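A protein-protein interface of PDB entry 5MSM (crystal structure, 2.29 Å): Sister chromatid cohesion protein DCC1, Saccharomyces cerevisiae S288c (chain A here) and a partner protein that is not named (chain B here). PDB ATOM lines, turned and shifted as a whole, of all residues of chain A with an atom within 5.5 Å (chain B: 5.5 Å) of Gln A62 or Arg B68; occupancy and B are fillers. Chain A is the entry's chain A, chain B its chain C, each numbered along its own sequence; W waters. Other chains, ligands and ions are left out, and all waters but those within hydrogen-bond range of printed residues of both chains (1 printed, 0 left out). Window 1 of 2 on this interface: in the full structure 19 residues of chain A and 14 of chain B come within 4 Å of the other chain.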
ATOM      1  N   LEU A  60      11.578 -36.790  22.094  1.00  0.00           N
ATOM      2  CA  LEU A  60      12.377 -35.710  21.546  1.00  0.00           C
ATOM      3  C   LEU A  60      11.567 -34.453  21.293  1.00  0.00           C
ATOM      4  O   LEU A  60      10.465 -34.518  20.761  1.00  0.00           O
ATOM      5  CB  LEU A  60      13.008 -36.141  20.240  1.00  0.00           C
ATOM      6  CG  LEU A  60      14.236 -37.005  20.377  1.00  0.00           C
ATOM      7  CD1 LEU A  60      14.652 -37.404  19.000  1.00  0.00           C
ATOM      8  CD2 LEU A  60      15.318 -36.186  21.018  1.00  0.00           C
ATOM      9  N   LYS A  61      12.118 -33.306  21.657  1.00  0.00           N
ATOM     10  CA  LYS A  61      11.513 -32.043  21.270  1.00  0.00           C
ATOM     11  C   LYS A  61      12.608 -31.137  20.756  1.00  0.00           C
ATOM     12  O   LYS A  61      13.764 -31.276  21.139  1.00  0.00           O
ATOM     13  CB  LYS A  61      10.776 -31.404  22.441  1.00  0.00           C
ATOM     14  CG  LYS A  61       9.644 -32.246  23.011  1.00  0.00           C
ATOM     15  CD  LYS A  61       8.484 -32.397  22.034  1.00  0.00           C
ATOM     16  CE  LYS A  61       7.310 -33.093  22.708  1.00  0.00           C
ATOM     17  NZ  LYS A  61       6.269 -33.501  21.733  1.00  0.00           N
ATOM     18  N   GLN A  62      12.278 -30.229  19.858  1.00  0.00           N
ATOM     19  CA  GLN A  62      13.296 -29.323  19.418  1.00  0.00           C
ATOM     20  C   GLN A  62      12.918 -27.885  19.762  1.00  0.00           C
ATOM     21  O   GLN A  62      11.749 -27.510  19.706  1.00  0.00           O
ATOM     22  CB  GLN A  62      13.559 -29.489  17.929  1.00  0.00           C
ATOM     23  CG  GLN A  62      12.465 -28.985  17.079  1.00  0.00           C
ATOM     24  CD  GLN A  62      12.655 -29.357  15.636  1.00  0.00           C
ATOM     25  OE1 GLN A  62      13.755 -29.179  15.084  1.00  0.00           O
ATOM     26  NE2 GLN A  62      11.570 -29.865  14.994  1.00  0.00           N
ATOM     27  N   ARG A  63      13.930 -27.112  20.155  1.00  0.00           N
ATOM     28  CA  ARG A  63      13.767 -25.734  20.589  1.00  0.00           C
ATOM     29  C   ARG A  63      14.776 -24.846  19.877  1.00  0.00           C
ATOM     30  O   ARG A  63      15.971 -24.926  20.143  1.00  0.00           O
ATOM     31  CB  ARG A  63      13.957 -25.611  22.103  1.00  0.00           C
ATOM     32  CG  ARG A  63      13.534 -24.264  22.663  1.00  0.00           C
ATOM     33  CD  ARG A  63      13.950 -24.099  24.116  1.00  0.00           C
ATOM     34  NE  ARG A  63      13.292 -25.072  24.967  1.00  0.00           N
ATOM     35  CZ  ARG A  63      12.034 -24.961  25.406  1.00  0.00           C
ATOM     36  NH1 ARG A  63      11.312 -23.880  25.099  1.00  0.00           N
ATOM     37  NH2 ARG A  63      11.516 -25.925  26.171  1.00  0.00           N
ATOM     38  N   LYS A  64      14.297 -24.013  18.965  1.00  0.00           N
ATOM     39  CA  LYS A  64      15.147 -23.035  18.303  1.00  0.00           C
ATOM     40  C   LYS A  64      15.563 -21.919  19.263  1.00  0.00           C
ATOM     41  O   LYS A  64      14.825 -21.592  20.199  1.00  0.00           O
ATOM     42  CB  LYS A  64      14.411 -22.450  17.092  1.00  0.00           C
ATOM     43  CG  LYS A  64      14.194 -23.475  15.999  1.00  0.00           C
ATOM     44  CD  LYS A  64      13.436 -22.905  14.807  1.00  0.00           C
ATOM     45  CE  LYS A  64      13.178 -24.008  13.776  1.00  0.00           C
ATOM     46  NZ  LYS A  64      12.415 -23.510  12.592  1.00  0.00           N
ATOM     47  N   SER A 106      19.271 -24.677  17.146  1.00  0.00           N
ATOM     48  CA  SER A 106      18.314 -25.348  18.026  1.00  0.00           C
ATOM     49  C   SER A 106      18.963 -26.512  18.752  1.00  0.00           C
ATOM     50  O   SER A 106      20.014 -26.981  18.331  1.00  0.00           O
ATOM     51  CB  SER A 106      17.119 -25.883  17.237  1.00  0.00           C
ATOM     52  OG  SER A 106      17.539 -26.970  16.435  1.00  0.00           O
ATOM     53  N   GLU A 107      18.340 -26.943  19.853  1.00  0.00           N
ATOM     54  CA  GLU A 107      18.693 -28.168  20.565  1.00  0.00           C
ATOM     55  C   GLU A 107      17.582 -29.207  20.478  1.00  0.00           C
ATOM     56  O   GLU A 107      16.390 -28.877  20.459  1.00  0.00           O
ATOM     57  CB  GLU A 107      19.003 -27.861  22.029  1.00  0.00           C
ATOM     58  CG  GLU A 107      20.226 -26.980  22.161  1.00  0.00           C
ATOM     59  CD  GLU A 107      20.651 -26.711  23.587  1.00  0.00           C
ATOM     60  OE1 GLU A 107      19.917 -27.051  24.547  1.00  0.00           O
ATOM     61  OE2 GLU A 107      21.739 -26.131  23.732  1.00  0.00           O
ATOM     62  N   PHE A 108      17.947 -30.473  20.429  1.00  0.00           N
ATOM     63  CA  PHE A 108      16.926 -31.485  20.606  1.00  0.00           C
ATOM     64  C   PHE A 108      16.907 -31.842  22.058  1.00  0.00           C
ATOM     65  O   PHE A 108      17.923 -32.241  22.604  1.00  0.00           O
ATOM     66  CB  PHE A 108      17.179 -32.674  19.687  1.00  0.00           C
ATOM     67  CG  PHE A 108      17.004 -32.306  18.248  1.00  0.00           C
ATOM     68  CD1 PHE A 108      17.909 -31.437  17.632  1.00  0.00           C
ATOM     69  CD2 PHE A 108      15.878 -32.695  17.556  1.00  0.00           C
ATOM     70  CE1 PHE A 108      17.733 -31.020  16.316  1.00  0.00           C
ATOM     71  CE2 PHE A 108      15.694 -32.287  16.242  1.00  0.00           C
ATOM     72  CZ  PHE A 108      16.631 -31.441  15.622  1.00  0.00           C
ATOM     73  N   GLU A 109      15.774 -31.593  22.709  1.00  0.00           N
ATOM     74  CA  GLU A 109      15.659 -31.834  24.142  1.00  0.00           C
ATOM     75  C   GLU A 109      15.087 -33.235  24.332  1.00  0.00           C
ATOM     76  O   GLU A 109      14.270 -33.682  23.535  1.00  0.00           O
ATOM     77  CB  GLU A 109      14.792 -30.765  24.816  1.00  0.00           C
ATOM     78  CG  GLU A 109      15.330 -29.334  24.704  1.00  0.00           C
ATOM     79  CD  GLU A 109      14.459 -28.297  25.420  1.00  0.00           C
ATOM     80  OE1 GLU A 109      13.280 -28.604  25.703  1.00  0.00           O
ATOM     81  OE2 GLU A 109      14.940 -27.164  25.688  1.00  0.00           O
ATOM     82  N   ARG A 111      13.134 -35.745  27.014  1.00  0.00           N
ATOM     83  CA  ARG A 111      12.345 -35.729  28.233  1.00  0.00           C
ATOM     84  C   ARG A 111      11.747 -37.115  28.512  1.00  0.00           C
ATOM     85  O   ARG A 111      11.223 -37.760  27.614  1.00  0.00           O
ATOM     86  CB  ARG A 111      11.262 -34.661  28.080  1.00  0.00           C
ATOM     87  CG  ARG A 111      11.480 -33.429  28.942  1.00  0.00           C
ATOM     88  CD  ARG A 111      10.250 -32.531  28.953  1.00  0.00           C
ATOM     89  NE  ARG A 111       9.011 -33.245  29.259  1.00  0.00           N
ATOM     90  CZ  ARG A 111       7.797 -32.772  28.990  1.00  0.00           C
ATOM     91  NH1 ARG A 111       7.650 -31.588  28.398  1.00  0.00           N
ATOM     92  NH2 ARG A 111       6.728 -33.487  29.305  1.00  0.00           N
ATOM     93  N   ALA B  66      12.873 -20.090  21.563  1.00  0.00           N
ATOM     94  CA  ALA B  66      11.499 -20.190  21.090  1.00  0.00           C
ATOM     95  C   ALA B  66      10.750 -21.289  21.844  1.00  0.00           C
ATOM     96  O   ALA B  66      11.312 -21.974  22.699  1.00  0.00           O
ATOM     97  CB  ALA B  66      11.453 -20.439  19.571  1.00  0.00           C
ATOM     98  N   VAL B  67       9.463 -21.430  21.545  1.00  0.00           N
ATOM     99  CA  VAL B  67       8.651 -22.445  22.184  1.00  0.00           C
ATOM    100  C   VAL B  67       9.144 -23.803  21.676  1.00  0.00           C
ATOM    101  O   VAL B  67       9.544 -23.913  20.514  1.00  0.00           O
ATOM    102  CB  VAL B  67       7.142 -22.209  21.854  1.00  0.00           C
ATOM    103  CG1 VAL B  67       6.467 -23.487  21.398  1.00  0.00           C
ATOM    104  CG2 VAL B  67       6.409 -21.544  23.031  1.00  0.00           C
ATOM    105  N   ARG B  68       9.141 -24.834  22.513  1.00  0.00           N
ATOM    106  CA  ARG B  68       9.543 -26.144  22.014  1.00  0.00           C
ATOM    107  C   ARG B  68       8.495 -26.753  21.064  1.00  0.00           C
ATOM    108  O   ARG B  68       7.295 -26.496  21.180  1.00  0.00           O
ATOM    109  CB  ARG B  68       9.838 -27.113  23.166  1.00  0.00           C
ATOM    110  CG  ARG B  68       8.638 -27.602  23.964  1.00  0.00           C
ATOM    111  CD  ARG B  68       9.054 -28.725  24.953  1.00  0.00           C
ATOM    112  NE  ARG B  68       7.999 -29.295  25.822  1.00  0.00           N
ATOM    113  CZ  ARG B  68       6.733 -29.571  25.485  1.00  0.00           C
ATOM    114  NH1 ARG B  68       6.245 -29.335  24.259  1.00  0.00           N
ATOM    115  NH2 ARG B  68       5.931 -30.099  26.409  1.00  0.00           N
ATOM    116  N   LYS B  69       8.979 -27.582  20.147  1.00  0.00           N
ATOM    117  CA  LYS B  69       8.168 -28.184  19.102  1.00  0.00           C
ATOM    118  C   LYS B  69       8.351 -29.698  19.010  1.00  0.00           C
ATOM    119  O   LYS B  69       9.414 -30.237  19.366  1.00  0.00           O
ATOM    120  CB  LYS B  69       8.519 -27.567  17.756  1.00  0.00           C
ATOM    121  CG  LYS B  69       8.296 -26.064  17.654  1.00  0.00           C
ATOM    122  CD  LYS B  69       6.913 -25.733  17.119  1.00  0.00           C
ATOM    123  CE  LYS B  69       6.789 -24.224  16.955  1.00  0.00           C
ATOM    124  NZ  LYS B  69       5.412 -23.754  16.662  1.00  0.00           N
ATOM    125  N   ASN B  70       7.338 -30.371  18.467  1.00  0.00           N
ATOM    126  CA  ASN B  70       7.420 -31.798  18.217  1.00  0.00           C
ATOM    127  C   ASN B  70       8.450 -32.138  17.139  1.00  0.00           C
ATOM    128  O   ASN B  70       8.840 -31.296  16.344  1.00  0.00           O
ATOM    129  CB  ASN B  70       6.045 -32.347  17.821  1.00  0.00           C
ATOM    130  CG  ASN B  70       5.016 -32.207  18.926  1.00  0.00           C
ATOM    131  OD1 ASN B  70       5.358 -32.039  20.099  1.00  0.00           O
ATOM    132  ND2 ASN B  70       3.741 -32.300  18.558  1.00  0.00           N
ATOM    133  N   VAL B  71       8.901 -33.385  17.141  1.00  0.00           N
ATOM    134  CA  VAL B  71       9.914 -33.854  16.202  1.00  0.00           C
ATOM    135  C   VAL B  71       9.424 -35.071  15.429  1.00  0.00           C
ATOM    136  O   VAL B  71       8.958 -36.076  15.986  1.00  0.00           O
ATOM    137  CB  VAL B  71      11.260 -34.196  16.916  1.00  0.00           C
ATOM    138  CG1 VAL B  71      12.291 -34.728  15.934  1.00  0.00           C
ATOM    139  CG2 VAL B  71      11.798 -32.991  17.638  1.00  0.00           C
ATOM    140  N   ASN B  75      12.437 -34.847  10.547  1.00  0.00           N
ATOM    141  CA  ASN B  75      13.236 -33.699  10.966  1.00  0.00           C
ATOM    142  C   ASN B  75      14.654 -34.148  11.321  1.00  0.00           C
ATOM    143  O   ASN B  75      15.565 -33.313  11.377  1.00  0.00           O
ATOM    144  CB  ASN B  75      12.688 -32.859  12.150  1.00  0.00           C
ATOM    145  CG  ASN B  75      11.219 -32.525  12.032  1.00  0.00           C
ATOM    146  OD1 ASN B  75      10.420 -33.373  12.224  1.00  0.00           O
ATOM    147  ND2 ASN B  75      10.901 -31.394  11.394  1.00  0.00           N
HETATM  148  O   HOH W   1      11.052 -24.357  18.523  1.00  0.00           O
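The backbone carbonyl oxygen (O) of Lys A61 is in hydrogen-bond range of the backbone NH (N) of Glu A109, 2.6 Å away. N of Arg A63 sits at hydrogen-bond distance from O of Glu A107, 3.0 Å away. The guanidinium group of Arg A63 lies within salt-bridge range of the side-chain carboxylate of Glu A109, at 2.8 Å.
Water W1 lies within hydrogen-bond range of O of Val B67 (2.5 Å), N of Lys A64 (3.3 Å) and O of Gln A62 (3.4 Å).
O of Gln A62 lies within hydrogen-bond range of N of Lys B69, at 2.8 Å. The backbone carbonyl oxygen (O) of Asn B70 is in hydrogen-bond range of the side-chain amide nitrogen (NE2) of Gln A62 (3.4 Å). The guanidinium group (NH1) of Arg A63 is in hydrogen-bond range of the backbone carbonyl oxygen (O) of Ala B66 (3.1 Å). N of Ala B66 is in hydrogen-bond range of O of Lys A64 (2.8 Å). The side-chain amide oxygen (OD1) of Asn B70 lies close to the side-chain amino group (NZ) of Lys A61, 2.4 Å away. The guanidinium group of Arg A111 lies close to the guanidinium group of Arg B68, 3.0 Å away.
Of the printed residues of chain B, Lys A61 touches Lys B69, Asn B70 and Val B71. Gln A62 touches just these residues of chain B: Arg B68, Lys B69, Asn B70, Val B71 and Asn B75. Of the printed residues of chain A, Ala B66 touches Arg A63 and Lys A64. Arg B68 touches three residues of chain A. The nearest residue of chain B that does not touch Gln A62 is Val B67 (4.3 Å). The nearest residue of chain A that does not touch Arg B68 is Lys A61 (4.1 Å).
Among the printed residues, pairs that only touch across the chains: Lys A61 with Lys B69 (3.4 Å), Gln A62 with Arg B68 (3.5 Å), Arg A63 with Arg B68 (3.5 Å), Gln A62 with Val B71 (3.6 Å), Lys A61 with Val B71 (3.7 Å), Leu A60 with Val B71 (3.7 Å) and Gln A62 with Asn B75 (3.97 Å).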
